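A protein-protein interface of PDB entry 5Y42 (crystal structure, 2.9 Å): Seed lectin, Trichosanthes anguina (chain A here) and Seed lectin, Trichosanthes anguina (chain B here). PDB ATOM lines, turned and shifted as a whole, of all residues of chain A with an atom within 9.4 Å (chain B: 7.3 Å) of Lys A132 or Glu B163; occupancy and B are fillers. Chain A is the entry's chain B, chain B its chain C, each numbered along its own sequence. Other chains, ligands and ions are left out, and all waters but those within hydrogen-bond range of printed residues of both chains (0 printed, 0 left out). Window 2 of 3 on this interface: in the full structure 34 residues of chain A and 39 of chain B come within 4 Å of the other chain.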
ATOM      1  N   GLY A  84     -28.146 -27.160  24.447  1.00  0.00           N
ATOM      2  CA  GLY A  84     -26.922 -26.412  24.730  1.00  0.00           C
ATOM      3  C   GLY A  84     -25.758 -27.315  25.061  1.00  0.00           C
ATOM      4  O   GLY A  84     -25.840 -28.526  24.926  1.00  0.00           O
ATOM      5  N   VAL A  85     -24.700 -26.703  25.558  1.00  0.00           N
ATOM      6  CA  VAL A  85     -23.469 -27.442  25.843  1.00  0.00           C
ATOM      7  C   VAL A  85     -23.623 -28.455  26.966  1.00  0.00           C
ATOM      8  O   VAL A  85     -23.261 -29.608  26.790  1.00  0.00           O
ATOM      9  CB  VAL A  85     -22.271 -26.509  26.108  1.00  0.00           C
ATOM     10  CG1 VAL A  85     -20.963 -27.302  26.242  1.00  0.00           C
ATOM     11  CG2 VAL A  85     -22.136 -25.550  24.964  1.00  0.00           C
ATOM     12  N   GLU A 124     -28.465 -24.946  13.266  1.00  0.00           N
ATOM     13  CA  GLU A 124     -27.033 -24.856  13.488  1.00  0.00           C
ATOM     14  C   GLU A 124     -26.652 -23.578  14.220  1.00  0.00           C
ATOM     15  O   GLU A 124     -25.899 -23.613  15.196  1.00  0.00           O
ATOM     16  CB  GLU A 124     -26.261 -24.880  12.176  1.00  0.00           C
ATOM     17  CG  GLU A 124     -24.745 -25.059  12.353  1.00  0.00           C
ATOM     18  CD  GLU A 124     -23.929 -24.754  11.096  1.00  0.00           C
ATOM     19  OE1 GLU A 124     -24.522 -24.263  10.089  1.00  0.00           O
ATOM     20  OE2 GLU A 124     -22.692 -25.003  11.116  1.00  0.00           O
ATOM     21  N   GLN A 125     -27.165 -22.442  13.742  1.00  0.00           N
ATOM     22  CA  GLN A 125     -26.820 -21.136  14.319  1.00  0.00           C
ATOM     23  C   GLN A 125     -27.381 -20.980  15.708  1.00  0.00           C
ATOM     24  O   GLN A 125     -26.717 -20.468  16.572  1.00  0.00           O
ATOM     25  CB  GLN A 125     -27.192 -19.976  13.409  1.00  0.00           C
ATOM     26  CG  GLN A 125     -26.550 -18.632  13.822  1.00  0.00           C
ATOM     27  CD  GLN A 125     -25.018 -18.652  13.888  1.00  0.00           C
ATOM     28  OE1 GLN A 125     -24.344 -18.942  12.908  1.00  0.00           O
ATOM     29  NE2 GLN A 125     -24.475 -18.329  15.052  1.00  0.00           N
ATOM     30  N   SER A 126     -28.598 -21.430  15.947  1.00  0.00           N
ATOM     31  CA  SER A 126     -29.129 -21.434  17.311  1.00  0.00           C
ATOM     32  C   SER A 126     -28.231 -22.225  18.267  1.00  0.00           C
ATOM     33  O   SER A 126     -27.903 -21.743  19.340  1.00  0.00           O
ATOM     34  CB  SER A 126     -30.536 -22.012  17.305  1.00  0.00           C
ATOM     35  OG  SER A 126     -31.406 -21.154  16.594  1.00  0.00           O
ATOM     36  N   VAL A 127     -27.779 -23.398  17.839  1.00  0.00           N
ATOM     37  CA  VAL A 127     -26.918 -24.204  18.682  1.00  0.00           C
ATOM     38  C   VAL A 127     -25.549 -23.531  18.895  1.00  0.00           C
ATOM     39  O   VAL A 127     -25.032 -23.491  20.018  1.00  0.00           O
ATOM     40  CB  VAL A 127     -26.750 -25.653  18.126  1.00  0.00           C
ATOM     41  CG1 VAL A 127     -25.769 -26.469  18.955  1.00  0.00           C
ATOM     42  CG2 VAL A 127     -28.071 -26.388  18.135  1.00  0.00           C
ATOM     43  N   ALA A 128     -24.973 -23.001  17.828  1.00  0.00           N
ATOM     44  CA  ALA A 128     -23.670 -22.314  17.907  1.00  0.00           C
ATOM     45  C   ALA A 128     -23.643 -21.193  18.920  1.00  0.00           C
ATOM     46  O   ALA A 128     -22.720 -21.098  19.695  1.00  0.00           O
ATOM     47  CB  ALA A 128     -23.319 -21.783  16.534  1.00  0.00           C
ATOM     48  N   TYR A 129     -24.746 -20.432  19.010  1.00  0.00           N
ATOM     49  CA  TYR A 129     -24.902 -19.398  20.036  1.00  0.00           C
ATOM     50  C   TYR A 129     -24.796 -19.941  21.462  1.00  0.00           C
ATOM     51  O   TYR A 129     -24.204 -19.283  22.339  1.00  0.00           O
ATOM     52  CB  TYR A 129     -26.251 -18.705  19.887  1.00  0.00           C
ATOM     53  CG  TYR A 129     -26.271 -17.621  18.866  1.00  0.00           C
ATOM     54  CD1 TYR A 129     -25.231 -16.677  18.800  1.00  0.00           C
ATOM     55  CD2 TYR A 129     -27.350 -17.493  17.992  1.00  0.00           C
ATOM     56  CE1 TYR A 129     -25.260 -15.668  17.872  1.00  0.00           C
ATOM     57  CE2 TYR A 129     -27.388 -16.479  17.058  1.00  0.00           C
ATOM     58  CZ  TYR A 129     -26.345 -15.576  17.016  1.00  0.00           C
ATOM     59  OH  TYR A 129     -26.380 -14.582  16.106  1.00  0.00           O
ATOM     60  N   SER A 130     -25.332 -21.137  21.669  1.00  0.00           N
ATOM     61  CA  SER A 130     -25.376 -21.774  22.995  1.00  0.00           C
ATOM     62  C   SER A 130     -23.984 -22.175  23.355  1.00  0.00           C
ATOM     63  O   SER A 130     -23.611 -22.169  24.528  1.00  0.00           O
ATOM     64  CB  SER A 130     -26.289 -23.027  22.934  1.00  0.00           C
ATOM     65  OG  SER A 130     -25.610 -24.178  22.410  1.00  0.00           O
ATOM     66  N   PHE A 131     -23.160 -22.566  22.379  1.00  0.00           N
ATOM     67  CA  PHE A 131     -21.741 -22.839  22.605  1.00  0.00           C
ATOM     68  C   PHE A 131     -20.950 -21.562  22.963  1.00  0.00           C
ATOM     69  O   PHE A 131     -20.124 -21.580  23.898  1.00  0.00           O
ATOM     70  CB  PHE A 131     -21.135 -23.469  21.318  1.00  0.00           C
ATOM     71  CG  PHE A 131     -21.195 -24.969  21.287  1.00  0.00           C
ATOM     72  CD1 PHE A 131     -22.367 -25.612  20.948  1.00  0.00           C
ATOM     73  CD2 PHE A 131     -20.080 -25.737  21.614  1.00  0.00           C
ATOM     74  CE1 PHE A 131     -22.436 -26.989  20.939  1.00  0.00           C
ATOM     75  CE2 PHE A 131     -20.146 -27.116  21.617  1.00  0.00           C
ATOM     76  CZ  PHE A 131     -21.323 -27.742  21.274  1.00  0.00           C
ATOM     77  N   LYS A 132     -21.104 -20.503  22.189  1.00  0.00           N
ATOM     78  CA  LYS A 132     -20.276 -19.314  22.252  1.00  0.00           C
ATOM     79  C   LYS A 132     -20.569 -18.566  23.519  1.00  0.00           C
ATOM     80  O   LYS A 132     -19.653 -18.248  24.274  1.00  0.00           O
ATOM     81  CB  LYS A 132     -20.548 -18.388  21.065  1.00  0.00           C
ATOM     82  CG  LYS A 132     -19.682 -17.144  21.097  1.00  0.00           C
ATOM     83  CD  LYS A 132     -19.475 -16.544  19.724  1.00  0.00           C
ATOM     84  CE  LYS A 132     -18.778 -15.203  19.853  1.00  0.00           C
ATOM     85  NZ  LYS A 132     -19.628 -14.202  20.564  1.00  0.00           N
ATOM     86  N   ASN A 133     -21.860 -18.311  23.736  1.00  0.00           N
ATOM     87  CA  ASN A 133     -22.353 -17.631  24.928  1.00  0.00           C
ATOM     88  C   ASN A 133     -22.479 -18.550  26.176  1.00  0.00           C
ATOM     89  O   ASN A 133     -22.798 -18.053  27.253  1.00  0.00           O
ATOM     90  CB  ASN A 133     -23.724 -16.999  24.647  1.00  0.00           C
ATOM     91  CG  ASN A 133     -23.714 -16.065  23.458  1.00  0.00           C
ATOM     92  OD1 ASN A 133     -22.776 -15.321  23.245  1.00  0.00           O
ATOM     93  ND2 ASN A 133     -24.776 -16.095  22.687  1.00  0.00           N
ATOM     94  N   GLU A 134     -22.240 -19.861  26.049  1.00  0.00           N
ATOM     95  CA  GLU A 134     -22.457 -20.811  27.141  1.00  0.00           C
ATOM     96  C   GLU A 134     -23.814 -20.567  27.798  1.00  0.00           C
ATOM     97  O   GLU A 134     -23.907 -20.351  28.991  1.00  0.00           O
ATOM     98  CB  GLU A 134     -21.307 -20.751  28.138  1.00  0.00           C
ATOM     99  CG  GLU A 134     -20.041 -21.402  27.597  1.00  0.00           C
ATOM    100  CD  GLU A 134     -18.835 -21.220  28.507  1.00  0.00           C
ATOM    101  OE1 GLU A 134     -18.685 -20.126  29.089  1.00  0.00           O
ATOM    102  OE2 GLU A 134     -18.025 -22.169  28.633  1.00  0.00           O
ATOM    103  N   LYS A 135     -24.857 -20.578  26.973  1.00  0.00           N
ATOM    104  CA  LYS A 135     -26.227 -20.311  27.406  1.00  0.00           C
ATOM    105  C   LYS A 135     -27.199 -21.219  26.660  1.00  0.00           C
ATOM    106  O   LYS A 135     -27.279 -21.174  25.426  1.00  0.00           O
ATOM    107  CB  LYS A 135     -26.591 -18.839  27.168  1.00  0.00           C
ATOM    108  CG  LYS A 135     -27.933 -18.455  27.763  1.00  0.00           C
ATOM    109  CD  LYS A 135     -28.305 -16.993  27.552  1.00  0.00           C
ATOM    110  CE  LYS A 135     -29.818 -16.814  27.482  1.00  0.00           C
ATOM    111  NZ  LYS A 135     -30.616 -17.711  28.384  1.00  0.00           N
ATOM    112  N   THR A 136     -27.908 -22.031  27.442  1.00  0.00           N
ATOM    113  CA  THR A 136     -28.914 -22.932  26.968  1.00  0.00           C
ATOM    114  C   THR A 136     -30.184 -22.226  26.411  1.00  0.00           C
ATOM    115  O   THR A 136     -30.446 -21.071  26.712  1.00  0.00           O
ATOM    116  CB  THR A 136     -29.350 -23.896  28.088  1.00  0.00           C
ATOM    117  OG1 THR A 136     -30.153 -23.207  29.056  1.00  0.00           O
ATOM    118  CG2 THR A 136     -28.115 -24.607  28.752  1.00  0.00           C
ATOM    119  N   PHE A 137     -30.899 -22.908  25.540  1.00  0.00           N
ATOM    120  CA  PHE A 137     -32.179 -22.415  24.992  1.00  0.00           C
ATOM    121  C   PHE A 137     -33.202 -23.540  24.883  1.00  0.00           C
ATOM    122  O   PHE A 137     -32.874 -24.727  24.935  1.00  0.00           O
ATOM    123  CB  PHE A 137     -31.937 -21.723  23.645  1.00  0.00           C
ATOM    124  CG  PHE A 137     -31.449 -22.640  22.555  1.00  0.00           C
ATOM    125  CD1 PHE A 137     -30.104 -23.018  22.484  1.00  0.00           C
ATOM    126  CD2 PHE A 137     -32.328 -23.109  21.583  1.00  0.00           C
ATOM    127  CE1 PHE A 137     -29.665 -23.869  21.463  1.00  0.00           C
ATOM    128  CE2 PHE A 137     -31.889 -23.940  20.566  1.00  0.00           C
ATOM    129  CZ  PHE A 137     -30.565 -24.335  20.509  1.00  0.00           C
ATOM    130  N   LEU B 145     -19.204 -14.256  10.337  1.00  0.00           N
ATOM    131  CA  LEU B 145     -18.076 -14.808  11.042  1.00  0.00           C
ATOM    132  C   LEU B 145     -17.997 -14.524  12.526  1.00  0.00           C
ATOM    133  O   LEU B 145     -18.448 -13.479  12.975  1.00  0.00           O
ATOM    134  CB  LEU B 145     -16.882 -14.191  10.342  1.00  0.00           C
ATOM    135  CG  LEU B 145     -15.491 -14.658  10.678  1.00  0.00           C
ATOM    136  CD1 LEU B 145     -15.262 -16.074  10.154  1.00  0.00           C
ATOM    137  CD2 LEU B 145     -14.527 -13.653  10.067  1.00  0.00           C
ATOM    138  N   ASP B 146     -17.527 -15.506  13.283  1.00  0.00           N
ATOM    139  CA  ASP B 146     -17.442 -15.485  14.731  1.00  0.00           C
ATOM    140  C   ASP B 146     -18.795 -15.281  15.390  1.00  0.00           C
ATOM    141  O   ASP B 146     -18.883 -14.832  16.514  1.00  0.00           O
ATOM    142  CB  ASP B 146     -16.431 -14.470  15.333  1.00  0.00           C
ATOM    143  CG  ASP B 146     -15.001 -14.656  14.833  1.00  0.00           C
ATOM    144  OD1 ASP B 146     -14.604 -15.814  14.589  1.00  0.00           O
ATOM    145  OD2 ASP B 146     -14.265 -13.627  14.700  1.00  0.00           O
ATOM    146  N   ASP B 147     -19.835 -15.683  14.685  1.00  0.00           N
ATOM    147  CA  ASP B 147     -21.220 -15.562  15.164  1.00  0.00           C
ATOM    148  C   ASP B 147     -21.667 -14.140  15.527  1.00  0.00           C
ATOM    149  O   ASP B 147     -22.447 -13.918  16.413  1.00  0.00           O
ATOM    150  CB  ASP B 147     -21.492 -16.470  16.391  1.00  0.00           C
ATOM    151  CG  ASP B 147     -21.080 -17.897  16.176  1.00  0.00           C
ATOM    152  OD1 ASP B 147     -21.658 -18.569  15.277  1.00  0.00           O
ATOM    153  OD2 ASP B 147     -20.182 -18.322  16.930  1.00  0.00           O
ATOM    154  N   MET B 148     -21.088 -13.209  14.822  1.00  0.00           N
ATOM    155  CA  MET B 148     -21.322 -11.787  14.970  1.00  0.00           C
ATOM    156  C   MET B 148     -22.412 -11.318  14.008  1.00  0.00           C
ATOM    157  O   MET B 148     -22.560 -11.859  12.932  1.00  0.00           O
ATOM    158  CB  MET B 148     -20.029 -10.993  14.759  1.00  0.00           C
ATOM    159  CG  MET B 148     -19.066 -11.229  15.899  1.00  0.00           C
ATOM    160  SD  MET B 148     -17.737 -10.041  15.951  1.00  0.00           S
ATOM    161  CE  MET B 148     -16.603 -10.987  16.981  1.00  0.00           C
ATOM    162  N   CYS B 149     -23.126 -10.253  14.387  1.00  0.00           N
ATOM    163  CA  CYS B 149     -24.248  -9.730  13.631  1.00  0.00           C
ATOM    164  C   CYS B 149     -23.873  -8.464  12.839  1.00  0.00           C
ATOM    165  O   CYS B 149     -23.204  -7.565  13.379  1.00  0.00           O
ATOM    166  CB  CYS B 149     -25.362  -9.390  14.605  1.00  0.00           C
ATOM    167  SG  CYS B 149     -26.168 -10.872  15.175  1.00  0.00           S
ATOM    168  N   GLU B 151     -24.446  -4.876  11.817  1.00  0.00           N
ATOM    169  CA  GLU B 151     -25.096  -3.748  12.467  1.00  0.00           C
ATOM    170  C   GLU B 151     -25.048  -2.465  11.639  1.00  0.00           C
ATOM    171  O   GLU B 151     -24.040  -2.169  10.987  1.00  0.00           O
ATOM    172  CB  GLU B 151     -24.442  -3.515  13.830  1.00  0.00           C
ATOM    173  CG  GLU B 151     -25.255  -2.644  14.776  1.00  0.00           C
ATOM    174  CD  GLU B 151     -24.702  -2.562  16.202  1.00  0.00           C
ATOM    175  OE1 GLU B 151     -24.644  -3.590  16.923  1.00  0.00           O
ATOM    176  OE2 GLU B 151     -24.339  -1.432  16.602  1.00  0.00           O
ATOM    177  N   TRP B 160     -21.206  -2.906   9.617  1.00  0.00           N
ATOM    178  CA  TRP B 160     -20.139  -3.848   9.924  1.00  0.00           C
ATOM    179  C   TRP B 160     -20.561  -4.789  11.063  1.00  0.00           C
ATOM    180  O   TRP B 160     -21.685  -4.672  11.584  1.00  0.00           O
ATOM    181  CB  TRP B 160     -18.786  -3.134  10.256  1.00  0.00           C
ATOM    182  CG  TRP B 160     -18.851  -2.194  11.437  1.00  0.00           C
ATOM    183  CD1 TRP B 160     -18.993  -2.533  12.759  1.00  0.00           C
ATOM    184  CD2 TRP B 160     -18.827  -0.768  11.391  1.00  0.00           C
ATOM    185  NE1 TRP B 160     -19.046  -1.402  13.535  1.00  0.00           N
ATOM    186  CE2 TRP B 160     -18.945  -0.306  12.720  1.00  0.00           C
ATOM    187  CE3 TRP B 160     -18.706   0.171  10.357  1.00  0.00           C
ATOM    188  CZ2 TRP B 160     -18.956   1.052  13.041  1.00  0.00           C
ATOM    189  CZ3 TRP B 160     -18.722   1.528  10.674  1.00  0.00           C
ATOM    190  CH2 TRP B 160     -18.839   1.954  12.005  1.00  0.00           C
ATOM    191  N   LEU B 161     -19.665  -5.705  11.419  1.00  0.00           N
ATOM    192  CA  LEU B 161     -19.977  -6.741  12.401  1.00  0.00           C
ATOM    193  C   LEU B 161     -19.740  -6.326  13.846  1.00  0.00           C
ATOM    194  O   LEU B 161     -18.675  -5.859  14.215  1.00  0.00           O
ATOM    195  CB  LEU B 161     -19.234  -8.043  12.100  1.00  0.00           C
ATOM    196  CG  LEU B 161     -19.686  -8.727  10.810  1.00  0.00           C
ATOM    197  CD1 LEU B 161     -18.786  -9.910  10.564  1.00  0.00           C
ATOM    198  CD2 LEU B 161     -21.142  -9.174  10.869  1.00  0.00           C
ATOM    199  N   GLU B 162     -20.765  -6.514  14.647  1.00  0.00           N
ATOM    200  CA  GLU B 162     -20.706  -6.328  16.085  1.00  0.00           C
ATOM    201  C   GLU B 162     -21.206  -7.599  16.749  1.00  0.00           C
ATOM    202  O   GLU B 162     -21.803  -8.457  16.111  1.00  0.00           O
ATOM    203  CB  GLU B 162     -21.575  -5.124  16.485  1.00  0.00           C
ATOM    204  CG  GLU B 162     -21.064  -3.768  15.981  1.00  0.00           C
ATOM    205  CD  GLU B 162     -19.834  -3.235  16.724  1.00  0.00           C
ATOM    206  OE1 GLU B 162     -19.447  -3.839  17.750  1.00  0.00           O
ATOM    207  OE2 GLU B 162     -19.249  -2.199  16.297  1.00  0.00           O
ATOM    208  N   GLU B 163     -20.876  -7.723  18.037  1.00  0.00           N
ATOM    209  CA  GLU B 163     -21.303  -8.822  18.887  1.00  0.00           C
ATOM    210  C   GLU B 163     -22.798  -8.776  18.992  1.00  0.00           C
ATOM    211  O   GLU B 163     -23.364  -7.731  19.289  1.00  0.00           O
ATOM    212  CB  GLU B 163     -20.728  -8.630  20.281  1.00  0.00           C
ATOM    213  CG  GLU B 163     -19.248  -8.961  20.368  1.00  0.00           C
ATOM    214  CD  GLU B 163     -19.023 -10.433  20.606  1.00  0.00           C
ATOM    215  OE1 GLU B 163     -19.859 -11.012  21.321  1.00  0.00           O
ATOM    216  OE2 GLU B 163     -18.029 -11.002  20.097  1.00  0.00           O
ATOM    217  N   CYS B 164     -23.484  -9.893  18.787  1.00  0.00           N
ATOM    218  CA  CYS B 164     -24.952  -9.866  18.768  1.00  0.00           C
ATOM    219  C   CYS B 164     -25.549  -9.556  20.104  1.00  0.00           C
ATOM    220  O   CYS B 164     -25.150 -10.126  21.075  1.00  0.00           O
ATOM    221  CB  CYS B 164     -25.570 -11.167  18.243  1.00  0.00           C
ATOM    222  SG  CYS B 164     -24.935 -11.666  16.618  1.00  0.00           S
ATOM    223  N   VAL B 165     -26.513  -8.634  20.117  1.00  0.00           N
ATOM    224  CA  VAL B 165     -27.259  -8.248  21.295  1.00  0.00           C
ATOM    225  C   VAL B 165     -28.733  -8.438  20.952  1.00  0.00           C
ATOM    226  O   VAL B 165     -29.285  -7.695  20.110  1.00  0.00           O
ATOM    227  CB  VAL B 165     -26.999  -6.767  21.647  1.00  0.00           C
ATOM    228  CG1 VAL B 165     -27.894  -6.310  22.800  1.00  0.00           C
ATOM    229  CG2 VAL B 165     -25.525  -6.555  21.977  1.00  0.00           C
ATOM    230  N   PRO B 166     -29.403  -9.383  21.622  1.00  0.00           N
ATOM    231  CA  PRO B 166     -30.791  -9.675  21.217  1.00  0.00           C
ATOM    232  C   PRO B 166     -31.719  -8.484  21.333  1.00  0.00           C
ATOM    233  O   PRO B 166     -31.626  -7.714  22.283  1.00  0.00           O
ATOM    234  CB  PRO B 166     -31.244 -10.776  22.179  1.00  0.00           C
ATOM    235  CG  PRO B 166     -30.009 -11.276  22.821  1.00  0.00           C
ATOM    236  CD  PRO B 166     -29.022 -10.142  22.820  1.00  0.00           C
ATOM    237  N   GLN B 168     -31.523  -5.713  19.751  1.00  0.00           N
ATOM    238  CA  GLN B 168     -30.908  -4.459  19.391  1.00  0.00           C
ATOM    239  C   GLN B 168     -31.529  -4.099  18.038  1.00  0.00           C
ATOM    240  O   GLN B 168     -31.676  -4.945  17.110  1.00  0.00           O
ATOM    241  CB  GLN B 168     -29.386  -4.521  19.302  1.00  0.00           C
ATOM    242  CG  GLN B 168     -28.768  -3.139  19.044  1.00  0.00           C
ATOM    243  CD  GLN B 168     -27.311  -2.965  19.506  1.00  0.00           C
ATOM    244  OE1 GLN B 168     -26.780  -3.762  20.278  1.00  0.00           O
ATOM    245  NE2 GLN B 168     -26.665  -1.900  19.030  1.00  0.00           N
ATOM    246  N   GLN B 171     -29.426  -4.063  14.583  1.00  0.00           N
ATOM    247  CA  GLN B 171     -29.055  -5.375  14.081  1.00  0.00           C
ATOM    248  C   GLN B 171     -30.231  -6.110  13.396  1.00  0.00           C
ATOM    249  O   GLN B 171     -30.089  -7.204  12.885  1.00  0.00           O
ATOM    250  CB  GLN B 171     -28.489  -6.257  15.221  1.00  0.00           C
ATOM    251  CG  GLN B 171     -27.137  -5.812  15.766  1.00  0.00           C
ATOM    252  CD  GLN B 171     -26.649  -6.626  16.964  1.00  0.00           C
ATOM    253  OE1 GLN B 171     -27.367  -7.481  17.483  1.00  0.00           O
ATOM    254  NE2 GLN B 171     -25.419  -6.367  17.398  1.00  0.00           N
ATOM    255  N   VAL B 242     -12.921  -8.873  11.689  1.00  0.00           N
ATOM    256  CA  VAL B 242     -14.058  -8.049  12.156  1.00  0.00           C
ATOM    257  C   VAL B 242     -13.612  -6.667  12.636  1.00  0.00           C
ATOM    258  O   VAL B 242     -14.363  -5.719  12.502  1.00  0.00           O
ATOM    259  CB  VAL B 242     -14.918  -8.697  13.259  1.00  0.00           C
ATOM    260  CG1 VAL B 242     -15.643  -9.911  12.717  1.00  0.00           C
ATOM    261  CG2 VAL B 242     -14.101  -9.049  14.490  1.00  0.00           C
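The side-chain carboxylate (OE1) of Glu B163 lies within salt-bridge range of the side-chain amino group (NZ) of Lys A132.
OD1 of Asp B147 lies within hydrogen-bond range of NE2 of Gln A125 (2.8 Å).
The side-chain hydroxyl of Tyr A129 lies within hydrogen-bond range of the side-chain sulfur of Cys B164 (3.3 Å).
The backbone carbonyl oxygen (O) of Tyr A129 is in hydrogen-bond range of the side-chain amide nitrogen (ND2) of Asn A133 (3.3 Å).
The backbone NH (N) of Cys B149 is in hydrogen-bond range of the backbone carbonyl oxygen (O) of Glu B162 (2.8 Å).
SG of Cys B149 is disulfide-bonded to SG of Cys B164, 2.1 Å away.
The backbone carbonyl oxygen (O) of Glu B163 is in hydrogen-bond range of the side-chain amide nitrogen (NE2) of Gln B171.
Among the printed residues, pairs that only touch across the chains: Ala A128 with Asp B147 (3.8 Å), Tyr A129 with Asp B147 (3.6 Å), Tyr A129 with Cys B149 (3.8 Å), Lys A132 with Asp B146 (3.4 Å) and Lys A132 with Asp B147 (3.4 Å).
Of the printed residues of chain B, Gln A125 touches Asp B147 (2.8 Å).
Of the printed residues of chain B, Ala A128 touches Asp B147.
Of chain B, only Asp B146, Asp B147 and Glu B163 come within 4 Å of Lys A132.
Of the printed residues of chain A, Asp B146 touches Lys A132.
Of the printed residues of chain A, Asp B147 touches Gln A125, Ala A128, Tyr A129 and Lys A132.
Printed residues of chain A within 4 Å of Cys B149: Tyr A129 (3.8 Å).
Of chain A, only Lys A132 comes within 4 Å of Glu B163.
The nearest printed residue of chain B that does not touch Tyr A129 is Met B148 (5.5 Å).
Along chain A the printed residues that touch a printed residue of chain B span positions 125 to 132.
Among the printed residues, 8 pairs touch across the chains.
Among the printed residues, Asp or Glu carboxylates within 4 Å of a Lys or Arg side-chain nitrogen of the other chain: Lys A132 with Glu B163.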
